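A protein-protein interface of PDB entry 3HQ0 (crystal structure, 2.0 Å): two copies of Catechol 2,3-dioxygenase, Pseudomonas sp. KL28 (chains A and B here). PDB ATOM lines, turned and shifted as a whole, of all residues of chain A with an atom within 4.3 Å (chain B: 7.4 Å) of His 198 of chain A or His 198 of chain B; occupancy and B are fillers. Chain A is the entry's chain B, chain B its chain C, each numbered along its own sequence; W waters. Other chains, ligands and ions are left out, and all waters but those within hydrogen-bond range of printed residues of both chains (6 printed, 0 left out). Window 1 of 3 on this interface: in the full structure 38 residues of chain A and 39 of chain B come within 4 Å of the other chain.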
ATOM      1  N   MET A   3      -5.211  15.286  21.593  1.00  0.00           N
ATOM      2  CA  MET A   3      -5.619  13.902  21.423  1.00  0.00           C
ATOM      3  C   MET A   3      -4.609  13.347  20.429  1.00  0.00           C
ATOM      4  O   MET A   3      -4.447  13.886  19.340  1.00  0.00           O
ATOM      5  CB  MET A   3      -7.036  13.803  20.852  1.00  0.00           C
ATOM      6  CG  MET A   3      -8.128  13.799  21.919  1.00  0.00           C
ATOM      7  SD  MET A   3      -7.981  12.363  23.021  1.00  0.00           S
ATOM      8  CE  MET A   3      -8.311  11.042  21.824  1.00  0.00           C
ATOM      9  N   TYR A 176      -5.730   3.925  29.445  1.00  0.00           N
ATOM     10  CA  TYR A 176      -5.546   3.932  30.889  1.00  0.00           C
ATOM     11  C   TYR A 176      -6.809   3.377  31.529  1.00  0.00           C
ATOM     12  O   TYR A 176      -7.894   3.435  30.937  1.00  0.00           O
ATOM     13  CB  TYR A 176      -5.220   5.347  31.404  1.00  0.00           C
ATOM     14  CG  TYR A 176      -6.331   6.375  31.291  1.00  0.00           C
ATOM     15  CD1 TYR A 176      -7.136   6.680  32.387  1.00  0.00           C
ATOM     16  CD2 TYR A 176      -6.565   7.052  30.095  1.00  0.00           C
ATOM     17  CE1 TYR A 176      -8.147   7.638  32.295  1.00  0.00           C
ATOM     18  CE2 TYR A 176      -7.574   8.008  29.993  1.00  0.00           C
ATOM     19  CZ  TYR A 176      -8.361   8.294  31.096  1.00  0.00           C
ATOM     20  OH  TYR A 176      -9.380   9.215  30.992  1.00  0.00           O
ATOM     21  N   SER A 195      -9.856   3.696  28.652  1.00  0.00           N
ATOM     22  CA  SER A 195     -10.111   4.884  27.840  1.00  0.00           C
ATOM     23  C   SER A 195      -8.820   5.315  27.150  1.00  0.00           C
ATOM     24  O   SER A 195      -7.739   5.070  27.661  1.00  0.00           O
ATOM     25  CB  SER A 195     -10.623   6.011  28.746  1.00  0.00           C
ATOM     26  OG  SER A 195     -10.656   7.262  28.083  1.00  0.00           O
ATOM     27  N   SER A 197      -8.922   8.495  25.725  1.00  0.00           N
ATOM     28  CA  SER A 197      -9.377   9.875  25.542  1.00  0.00           C
ATOM     29  C   SER A 197      -9.784  10.398  26.911  1.00  0.00           C
ATOM     30  O   SER A 197      -9.140  10.091  27.920  1.00  0.00           O
ATOM     31  CB  SER A 197     -10.606   9.867  24.634  1.00  0.00           C
ATOM     32  OG  SER A 197     -11.599   8.983  25.155  1.00  0.00           O
ATOM     33  N   HIS A 198     -10.840  11.203  26.955  1.00  0.00           N
ATOM     34  CA  HIS A 198     -11.322  11.653  28.250  1.00  0.00           C
ATOM     35  C   HIS A 198     -12.752  11.154  28.474  1.00  0.00           C
ATOM     36  O   HIS A 198     -13.533  11.734  29.227  1.00  0.00           O
ATOM     37  CB  HIS A 198     -11.174  13.182  28.455  1.00  0.00           C
ATOM     38  CG  HIS A 198     -11.911  14.034  27.468  1.00  0.00           C
ATOM     39  ND1 HIS A 198     -11.288  14.637  26.396  1.00  0.00           N
ATOM     40  CD2 HIS A 198     -13.199  14.446  27.433  1.00  0.00           C
ATOM     41  CE1 HIS A 198     -12.159  15.386  25.746  1.00  0.00           C
ATOM     42  NE2 HIS A 198     -13.326  15.288  26.354  1.00  0.00           N
ATOM     43  N   LYS A 199     -13.068  10.040  27.808  1.00  0.00           N
ATOM     44  CA  LYS A 199     -14.364   9.375  27.944  1.00  0.00           C
ATOM     45  C   LYS A 199     -14.214   8.328  29.055  1.00  0.00           C
ATOM     46  O   LYS A 199     -13.093   7.909  29.364  1.00  0.00           O
ATOM     47  CB  LYS A 199     -14.753   8.668  26.642  1.00  0.00           C
ATOM     48  CG  LYS A 199     -14.927   9.591  25.444  1.00  0.00           C
ATOM     49  CD  LYS A 199     -15.727   8.915  24.344  1.00  0.00           C
ATOM     50  CE  LYS A 199     -15.063   7.654  23.836  1.00  0.00           C
ATOM     51  NZ  LYS A 199     -16.010   6.816  23.045  1.00  0.00           N
ATOM     52  N   VAL A 200     -15.327   7.895  29.650  1.00  0.00           N
ATOM     53  CA  VAL A 200     -15.249   6.899  30.716  1.00  0.00           C
ATOM     54  C   VAL A 200     -14.625   5.616  30.183  1.00  0.00           C
ATOM     55  O   VAL A 200     -13.886   4.942  30.892  1.00  0.00           O
ATOM     56  CB  VAL A 200     -16.633   6.608  31.350  1.00  0.00           C
ATOM     57  CG1 VAL A 200     -17.128   7.849  32.077  1.00  0.00           C
ATOM     58  CG2 VAL A 200     -17.630   6.175  30.285  1.00  0.00           C
ATOM     59  N   HIS A 274     -16.073  12.633  33.303  1.00  0.00           N
ATOM     60  CA  HIS A 274     -15.041  13.035  32.359  1.00  0.00           C
ATOM     61  C   HIS A 274     -13.630  12.786  32.868  1.00  0.00           C
ATOM     62  O   HIS A 274     -12.944  13.699  33.336  1.00  0.00           O
ATOM     63  CB  HIS A 274     -15.250  14.506  32.023  1.00  0.00           C
ATOM     64  CG  HIS A 274     -16.662  14.823  31.648  1.00  0.00           C
ATOM     65  ND1 HIS A 274     -17.193  14.495  30.419  1.00  0.00           N
ATOM     66  CD2 HIS A 274     -17.686  15.328  32.378  1.00  0.00           C
ATOM     67  CE1 HIS A 274     -18.483  14.781  30.410  1.00  0.00           C
ATOM     68  NE2 HIS A 274     -18.808  15.285  31.587  1.00  0.00           N
ATOM     69  N   PRO A 275     -13.183  11.530  32.794  1.00  0.00           N
ATOM     70  CA  PRO A 275     -11.840  11.177  33.256  1.00  0.00           C
ATOM     71  C   PRO A 275     -10.739  11.648  32.317  1.00  0.00           C
ATOM     72  O   PRO A 275     -10.966  11.911  31.138  1.00  0.00           O
ATOM     73  CB  PRO A 275     -11.903   9.654  33.354  1.00  0.00           C
ATOM     74  CG  PRO A 275     -12.838   9.298  32.227  1.00  0.00           C
ATOM     75  CD  PRO A 275     -13.926  10.335  32.354  1.00  0.00           C
ATOM     76  N   TYR A 276      -9.542  11.760  32.866  1.00  0.00           N
ATOM     77  CA  TYR A 276      -8.372  12.165  32.106  1.00  0.00           C
ATOM     78  C   TYR A 276      -7.240  11.250  32.545  1.00  0.00           C
ATOM     79  O   TYR A 276      -7.283  10.679  33.626  1.00  0.00           O
ATOM     80  CB  TYR A 276      -8.011  13.621  32.398  1.00  0.00           C
ATOM     81  CG  TYR A 276      -8.902  14.616  31.698  1.00  0.00           C
ATOM     82  CD1 TYR A 276      -8.514  15.204  30.496  1.00  0.00           C
ATOM     83  CD2 TYR A 276     -10.142  14.960  32.236  1.00  0.00           C
ATOM     84  CE1 TYR A 276      -9.342  16.116  29.848  1.00  0.00           C
ATOM     85  CE2 TYR A 276     -10.977  15.861  31.597  1.00  0.00           C
ATOM     86  CZ  TYR A 276     -10.575  16.437  30.407  1.00  0.00           C
ATOM     87  OH  TYR A 276     -11.409  17.333  29.775  1.00  0.00           O
ATOM     88  N   ALA B   2      -4.871   8.583  22.795  1.00  0.00           N
ATOM     89  CA  ALA B   2      -4.604   9.051  24.186  1.00  0.00           C
ATOM     90  C   ALA B   2      -4.586  10.572  24.289  1.00  0.00           C
ATOM     91  O   ALA B   2      -4.342  11.271  23.299  1.00  0.00           O
ATOM     92  CB  ALA B   2      -3.254   8.499  24.660  1.00  0.00           C
ATOM     93  N   MET B   3      -4.841  11.073  25.494  1.00  0.00           N
ATOM     94  CA  MET B   3      -4.795  12.507  25.764  1.00  0.00           C
ATOM     95  C   MET B   3      -3.369  12.792  26.258  1.00  0.00           C
ATOM     96  O   MET B   3      -2.933  12.237  27.270  1.00  0.00           O
ATOM     97  CB  MET B   3      -5.805  12.884  26.850  1.00  0.00           C
ATOM     98  CG  MET B   3      -7.221  13.135  26.348  1.00  0.00           C
ATOM     99  SD  MET B   3      -7.263  14.577  25.263  1.00  0.00           S
ATOM    100  CE  MET B   3      -7.059  15.897  26.459  1.00  0.00           C
ATOM    101  N   LEU B   7      -3.811  18.853  28.568  1.00  0.00           N
ATOM    102  CA  LEU B   7      -5.014  18.055  28.805  1.00  0.00           C
ATOM    103  C   LEU B   7      -6.336  18.805  28.878  1.00  0.00           C
ATOM    104  O   LEU B   7      -7.299  18.452  28.189  1.00  0.00           O
ATOM    105  CB  LEU B   7      -4.847  17.246  30.085  1.00  0.00           C
ATOM    106  CG  LEU B   7      -3.634  16.322  30.190  1.00  0.00           C
ATOM    107  CD1 LEU B   7      -3.753  15.517  31.472  1.00  0.00           C
ATOM    108  CD2 LEU B   7      -3.556  15.402  28.977  1.00  0.00           C
ATOM    109  N   ARG B   8      -6.408  19.816  29.732  1.00  0.00           N
ATOM    110  CA  ARG B   8      -7.652  20.564  29.862  1.00  0.00           C
ATOM    111  C   ARG B   8      -7.492  21.818  30.696  1.00  0.00           C
ATOM    112  O   ARG B   8      -6.441  22.048  31.292  1.00  0.00           O
ATOM    113  CB  ARG B   8      -8.724  19.691  30.521  1.00  0.00           C
ATOM    114  CG  ARG B   8      -8.695  19.671  32.048  1.00  0.00           C
ATOM    115  CD  ARG B   8      -7.805  18.579  32.578  1.00  0.00           C
ATOM    116  NE  ARG B   8      -7.844  18.432  34.036  1.00  0.00           N
ATOM    117  CZ  ARG B   8      -7.246  17.428  34.675  1.00  0.00           C
ATOM    118  NH1 ARG B   8      -6.594  16.517  33.971  1.00  0.00           N
ATOM    119  NH2 ARG B   8      -7.273  17.337  35.996  1.00  0.00           N
ATOM    120  N   GLN B 151     -17.582  20.706  35.755  1.00  0.00           N
ATOM    121  CA  GLN B 151     -16.181  21.030  35.500  1.00  0.00           C
ATOM    122  C   GLN B 151     -16.046  22.424  34.918  1.00  0.00           C
ATOM    123  O   GLN B 151     -17.014  22.998  34.403  1.00  0.00           O
ATOM    124  CB  GLN B 151     -15.559  20.047  34.493  1.00  0.00           C
ATOM    125  CG  GLN B 151     -16.250  20.064  33.129  1.00  0.00           C
ATOM    126  CD  GLN B 151     -15.477  19.345  32.030  1.00  0.00           C
ATOM    127  OE1 GLN B 151     -15.052  18.197  32.185  1.00  0.00           O
ATOM    128  NE2 GLN B 151     -15.306  20.017  30.907  1.00  0.00           N
ATOM    129  N   TYR B 176      -6.428  22.689  18.236  1.00  0.00           N
ATOM    130  CA  TYR B 176      -6.889  22.667  16.855  1.00  0.00           C
ATOM    131  C   TYR B 176      -8.238  23.388  16.756  1.00  0.00           C
ATOM    132  O   TYR B 176      -9.060  23.311  17.667  1.00  0.00           O
ATOM    133  CB  TYR B 176      -6.991  21.226  16.353  1.00  0.00           C
ATOM    134  CG  TYR B 176      -8.100  20.394  16.967  1.00  0.00           C
ATOM    135  CD1 TYR B 176      -9.296  20.191  16.281  1.00  0.00           C
ATOM    136  CD2 TYR B 176      -7.942  19.789  18.216  1.00  0.00           C
ATOM    137  CE1 TYR B 176     -10.307  19.404  16.816  1.00  0.00           C
ATOM    138  CE2 TYR B 176      -8.951  19.001  18.765  1.00  0.00           C
ATOM    139  CZ  TYR B 176     -10.132  18.813  18.054  1.00  0.00           C
ATOM    140  OH  TYR B 176     -11.140  18.041  18.570  1.00  0.00           O
ATOM    141  N   VAL B 178     -11.944  24.151  15.997  1.00  0.00           N
ATOM    142  CA  VAL B 178     -13.165  23.363  15.814  1.00  0.00           C
ATOM    143  C   VAL B 178     -14.204  24.178  15.050  1.00  0.00           C
ATOM    144  O   VAL B 178     -14.891  23.664  14.165  1.00  0.00           O
ATOM    145  CB  VAL B 178     -13.791  22.923  17.158  1.00  0.00           C
ATOM    146  CG1 VAL B 178     -14.884  21.911  16.891  1.00  0.00           C
ATOM    147  CG2 VAL B 178     -12.730  22.336  18.081  1.00  0.00           C
ATOM    148  N   SER B 195      -9.790  23.499  20.679  1.00  0.00           N
ATOM    149  CA  SER B 195      -9.856  22.270  21.462  1.00  0.00           C
ATOM    150  C   SER B 195      -8.492  21.605  21.556  1.00  0.00           C
ATOM    151  O   SER B 195      -7.729  21.606  20.592  1.00  0.00           O
ATOM    152  CB  SER B 195     -10.828  21.274  20.822  1.00  0.00           C
ATOM    153  OG  SER B 195     -10.844  20.041  21.535  1.00  0.00           O
ATOM    154  N   CYS B 196      -8.191  21.043  22.721  1.00  0.00           N
ATOM    155  CA  CYS B 196      -6.950  20.304  22.918  1.00  0.00           C
ATOM    156  C   CYS B 196      -7.359  18.895  23.354  1.00  0.00           C
ATOM    157  O   CYS B 196      -6.606  18.180  24.016  1.00  0.00           O
ATOM    158  CB  CYS B 196      -6.084  20.970  23.994  1.00  0.00           C
ATOM    159  SG  CYS B 196      -6.802  21.045  25.635  1.00  0.00           S
ATOM    160  N   SER B 197      -8.562  18.500  22.942  1.00  0.00           N
ATOM    161  CA  SER B 197      -9.129  17.207  23.307  1.00  0.00           C
ATOM    162  C   SER B 197     -10.205  16.834  22.299  1.00  0.00           C
ATOM    163  O   SER B 197     -10.051  17.082  21.102  1.00  0.00           O
ATOM    164  CB  SER B 197      -9.763  17.322  24.690  1.00  0.00           C
ATOM    165  OG  SER B 197     -10.785  18.320  24.690  1.00  0.00           O
ATOM    166  N   HIS B 198     -11.282  16.207  22.768  1.00  0.00           N
ATOM    167  CA  HIS B 198     -12.379  15.896  21.869  1.00  0.00           C
ATOM    168  C   HIS B 198     -13.651  16.606  22.329  1.00  0.00           C
ATOM    169  O   HIS B 198     -14.770  16.153  22.105  1.00  0.00           O
ATOM    170  CB  HIS B 198     -12.588  14.378  21.671  1.00  0.00           C
ATOM    171  CG  HIS B 198     -12.983  13.625  22.901  1.00  0.00           C
ATOM    172  ND1 HIS B 198     -12.064  13.007  23.721  1.00  0.00           N
ATOM    173  CD2 HIS B 198     -14.200  13.328  23.412  1.00  0.00           C
ATOM    174  CE1 HIS B 198     -12.697  12.360  24.682  1.00  0.00           C
ATOM    175  NE2 HIS B 198     -13.995  12.539  24.517  1.00  0.00           N
ATOM    176  N   LYS B 199     -13.438  17.754  22.964  1.00  0.00           N
ATOM    177  CA  LYS B 199     -14.504  18.644  23.433  1.00  0.00           C
ATOM    178  C   LYS B 199     -14.626  19.687  22.318  1.00  0.00           C
ATOM    179  O   LYS B 199     -13.649  19.925  21.604  1.00  0.00           O
ATOM    180  CB  LYS B 199     -14.082  19.353  24.726  1.00  0.00           C
ATOM    181  CG  LYS B 199     -14.171  18.518  25.995  1.00  0.00           C
ATOM    182  CD  LYS B 199     -13.433  19.184  27.165  1.00  0.00           C
ATOM    183  CE  LYS B 199     -13.915  20.608  27.435  1.00  0.00           C
ATOM    184  NZ  LYS B 199     -13.040  21.303  28.441  1.00  0.00           N
ATOM    185  N   VAL B 200     -15.800  20.305  22.166  1.00  0.00           N
ATOM    186  CA  VAL B 200     -16.010  21.327  21.134  1.00  0.00           C
ATOM    187  C   VAL B 200     -15.004  22.460  21.292  1.00  0.00           C
ATOM    188  O   VAL B 200     -14.550  23.035  20.304  1.00  0.00           O
ATOM    189  CB  VAL B 200     -17.443  21.910  21.188  1.00  0.00           C
ATOM    190  CG1 VAL B 200     -17.608  22.997  20.125  1.00  0.00           C
ATOM    191  CG2 VAL B 200     -18.450  20.811  20.954  1.00  0.00           C
ATOM    192  N   HIS B 201     -14.694  22.815  22.536  1.00  0.00           N
ATOM    193  CA  HIS B 201     -13.670  23.821  22.801  1.00  0.00           C
ATOM    194  C   HIS B 201     -13.260  23.898  24.259  1.00  0.00           C
ATOM    195  O   HIS B 201     -14.087  23.776  25.168  1.00  0.00           O
ATOM    196  CB  HIS B 201     -14.063  25.216  22.282  1.00  0.00           C
ATOM    197  CG  HIS B 201     -15.149  25.891  23.059  1.00  0.00           C
ATOM    198  ND1 HIS B 201     -16.374  25.307  23.296  1.00  0.00           N
ATOM    199  CD2 HIS B 201     -15.217  27.137  23.591  1.00  0.00           C
ATOM    200  CE1 HIS B 201     -17.151  26.163  23.936  1.00  0.00           C
ATOM    201  NE2 HIS B 201     -16.475  27.282  24.125  1.00  0.00           N
ATOM    202  N   ASP B 202     -11.957  24.059  24.465  1.00  0.00           N
ATOM    203  CA  ASP B 202     -11.382  24.184  25.793  1.00  0.00           C
ATOM    204  C   ASP B 202     -11.143  25.666  26.070  1.00  0.00           C
ATOM    205  O   ASP B 202     -10.945  26.075  27.211  1.00  0.00           O
ATOM    206  CB  ASP B 202     -10.070  23.415  25.862  1.00  0.00           C
ATOM    207  CG  ASP B 202     -10.283  21.915  25.799  1.00  0.00           C
ATOM    208  OD1 ASP B 202     -10.802  21.360  26.788  1.00  0.00           O
ATOM    209  OD2 ASP B 202      -9.950  21.299  24.766  1.00  0.00           O
ATOM    210  N   TYR B 273     -21.192  18.567  19.949  1.00  0.00           N
ATOM    211  CA  TYR B 273     -20.827  17.344  19.249  1.00  0.00           C
ATOM    212  C   TYR B 273     -19.501  16.817  19.771  1.00  0.00           C
ATOM    213  O   TYR B 273     -19.053  17.224  20.846  1.00  0.00           O
ATOM    214  CB  TYR B 273     -20.786  17.584  17.736  1.00  0.00           C
ATOM    215  CG  TYR B 273     -20.084  18.850  17.318  1.00  0.00           C
ATOM    216  CD1 TYR B 273     -18.712  18.854  17.049  1.00  0.00           C
ATOM    217  CD2 TYR B 273     -20.783  20.053  17.207  1.00  0.00           C
ATOM    218  CE1 TYR B 273     -18.056  20.018  16.687  1.00  0.00           C
ATOM    219  CE2 TYR B 273     -20.133  21.224  16.845  1.00  0.00           C
ATOM    220  CZ  TYR B 273     -18.767  21.197  16.588  1.00  0.00           C
ATOM    221  OH  TYR B 273     -18.105  22.354  16.250  1.00  0.00           O
ATOM    222  N   HIS B 274     -18.858  15.936  19.013  1.00  0.00           N
ATOM    223  CA  HIS B 274     -17.614  15.338  19.483  1.00  0.00           C
ATOM    224  C   HIS B 274     -16.462  15.374  18.493  1.00  0.00           C
ATOM    225  O   HIS B 274     -16.093  14.352  17.912  1.00  0.00           O
ATOM    226  CB  HIS B 274     -17.902  13.898  19.896  1.00  0.00           C
ATOM    227  CG  HIS B 274     -19.030  13.778  20.873  1.00  0.00           C
ATOM    228  ND1 HIS B 274     -18.888  14.075  22.212  1.00  0.00           N
ATOM    229  CD2 HIS B 274     -20.335  13.464  20.690  1.00  0.00           C
ATOM    230  CE1 HIS B 274     -20.059  13.950  22.812  1.00  0.00           C
ATOM    231  NE2 HIS B 274     -20.953  13.581  21.912  1.00  0.00           N
ATOM    232  N   PRO B 275     -15.856  16.551  18.314  1.00  0.00           N
ATOM    233  CA  PRO B 275     -14.740  16.697  17.383  1.00  0.00           C
ATOM    234  C   PRO B 275     -13.464  16.006  17.826  1.00  0.00           C
ATOM    235  O   PRO B 275     -13.221  15.810  19.014  1.00  0.00           O
ATOM    236  CB  PRO B 275     -14.561  18.204  17.302  1.00  0.00           C
ATOM    237  CG  PRO B 275     -14.862  18.633  18.708  1.00  0.00           C
ATOM    238  CD  PRO B 275     -16.118  17.824  19.018  1.00  0.00           C
ATOM    239  N   TYR B 276     -12.653  15.649  16.837  1.00  0.00           N
ATOM    240  CA  TYR B 276     -11.367  15.012  17.048  1.00  0.00           C
ATOM    241  C   TYR B 276     -10.390  15.771  16.132  1.00  0.00           C
ATOM    242  O   TYR B 276     -10.810  16.414  15.166  1.00  0.00           O
ATOM    243  CB  TYR B 276     -11.460  13.523  16.695  1.00  0.00           C
ATOM    244  CG  TYR B 276     -12.103  12.660  17.781  1.00  0.00           C
ATOM    245  CD1 TYR B 276     -11.337  12.105  18.810  1.00  0.00           C
ATOM    246  CD2 TYR B 276     -13.482  12.411  17.784  1.00  0.00           C
ATOM    247  CE1 TYR B 276     -11.930  11.314  19.823  1.00  0.00           C
ATOM    248  CE2 TYR B 276     -14.083  11.628  18.788  1.00  0.00           C
ATOM    249  CZ  TYR B 276     -13.300  11.082  19.802  1.00  0.00           C
ATOM    250  OH  TYR B 276     -13.884  10.304  20.784  1.00  0.00           O
ATOM    251  N   PRO B 277      -9.082  15.718  16.428  1.00  0.00           N
ATOM    252  CA  PRO B 277      -8.041  16.403  15.646  1.00  0.00           C
ATOM    253  C   PRO B 277      -8.051  16.144  14.135  1.00  0.00           C
ATOM    254  O   PRO B 277      -7.512  16.934  13.361  1.00  0.00           O
ATOM    255  CB  PRO B 277      -6.741  15.926  16.298  1.00  0.00           C
ATOM    256  CG  PRO B 277      -7.148  15.605  17.690  1.00  0.00           C
ATOM    257  CD  PRO B 277      -8.481  14.933  17.518  1.00  0.00           C
HETATM  258  O   HOH W   1     -12.368   8.462  21.977  1.00  0.00           O
HETATM  259  O   HOH W   2     -15.644   8.030  20.442  1.00  0.00           O
HETATM  260  O   HOH W   3      -9.938  18.807  27.788  1.00  0.00           O
HETATM  261  O   HOH W   4      -6.876  16.905  20.252  1.00  0.00           O
HETATM  262  O   HOH W   5     -14.207  16.848  30.029  1.00  0.00           O
HETATM  263  O   HOH W   6     -12.200  19.699  30.787  1.00  0.00           O
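Of the 10 printed residues of chain A, 6 touch a printed residue of chain B.
Hydrophobic or aromatic side chains of chain B that line the printed part of chain A: Met 3, His 198 and Pro 277.
Among the printed residues, 14 pairs touch across the chains.
Among the printed residues, no Asp or Glu carboxylate lies within 4 Å of a Lys or Arg side-chain nitrogen of the other chain.
Water W1 bridges OH of Tyr 276 of chain B and OG of Ser 197 of chain A.
Water W5 bridges the side-chain amide oxygen of Gln 151 of chain B (2.7 Å) and the side-chain hydroxyl of Tyr 276 of chain A (2.9 Å).
Water W4 bridges N of Met 3 of chain A and O of Ser 197 of chain B.
Water W6 lies within hydrogen-bond range of the side-chain hydroxyl of Tyr 276 of chain A (2.7 Å), the side-chain amino group of Lys 199 of chain B (3.0 Å) and the side-chain amide nitrogen of Gln 151 of chain B (3.1 Å).
Water W3 lies within hydrogen-bond range of O of Leu 7 of chain B, OD1 of Asp 202 of chain B, OH of Tyr 276 of chain A and OG of Ser 197 of chain B.
Water W2 bridges NZ of Lys 199 of chain A (2.9 Å) and OH of Tyr 276 of chain B (2.9 Å).
The side-chain hydroxyl (OH) of Tyr 176 of chain A lies within hydrogen-bond range of the backbone NH (N) of Tyr 276 of chain A.
The side-chain hydroxyl (OG) of Ser 195 of chain B is in hydrogen-bond range of the backbone carbonyl oxygen (O) of Lys 199 of chain B.
OG of Ser 195 of chain B sits at hydrogen-bond distance from N of Ser 197 of chain B.
The side-chain hydroxyl of Ser 197 of chain A lies within hydrogen-bond range of the backbone NH of Lys 199 of chain A.
OG of Ser 195 of chain A lies within hydrogen-bond range of N of Ser 197 of chain A (3.2 Å).
The side-chain amino group of Lys 199 of chain B lies within salt-bridge range of the side-chain carboxylate of Asp 202 of chain B, at 2.8 Å.
Met 3 of chain A touches Ser 197 of chain B, and with the chains exchanged Ser 197 of chain A touches Met 3 of chain B.
Ser 197 of chain A touches His 198 of chain B, and with the chains exchanged His 198 of chain A touches Ser 197 of chain B.
His 198 of chain A touches its own counterpart, His 198 of chain B.
His 198 of chain A touches Lys 199 of chain B, and with the chains exchanged Lys 199 of chain A touches His 198 of chain B.
Positions printed for both chains: 3, 176, 195, 197, 198, 199, 200, 274, 275 and 276.
Of the 14 pairs that touch across the chains among the printed residues, 8 have their exchanged pair printed and touching as well.
Of the printed residues of chain B, Met 3 of chain A touches Ala 2, Met 3, Ser 197 and Pro 277.
Tyr 176 of chain A touches none of the printed residues of chain B.
Of chain B, only Ser 197, His 198 and Lys 199 come within 4 Å of His 198 of chain A.
Pro 275 of chain A touches none of the printed residues of chain B.
Of the printed residues of chain A, Met 3 of chain B touches Met 3 (3.2 Å) and Ser 197 (3.8 Å).
Of the printed residues of chain A, Arg 8 of chain B touches Tyr 276.
Printed residues of chain A within 4 Å of Ser 197 of chain B: Met 3 (3.7 Å) and His 198 (3.3 Å).
His 198 of chain B touches three residues of chain A.
The nearest residue of chain B that does not touch His 198 of chain A is Met 3 of chain B (4.1 Å).
A ring nitrogen (ND1) of His 198 of chain A sits close to a ring nitrogen (ND1) of His 198 of chain B (3.2 Å).
SD of Met 3 of chain B lies close to SD of Met 3 of chain A (3.2 Å).
Among the printed residues, pairs that only touch across the chains: Met 3 of chain A with Ala 2 of chain B, Met 3 of chain A with Ser 197 of chain B, Met 3 of chain A with Pro 277 of chain B, Ser 197 of chain A with Met 3 of chain B, Ser 197 of chain A with His 198 of chain B, His 198 of chain A with Ser 197 of chain B, His 198 of chain A with Lys 199 of chain B, Lys 199 of chain A with His 198 of chain B, His 274 of chain A with Gln 151 of chain B, Tyr 276 of chain A with Leu 7 of chain B, Tyr 276 of chain A with Arg 8 of chain B and Tyr 276 of chain A with Lys 199 of chain B.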
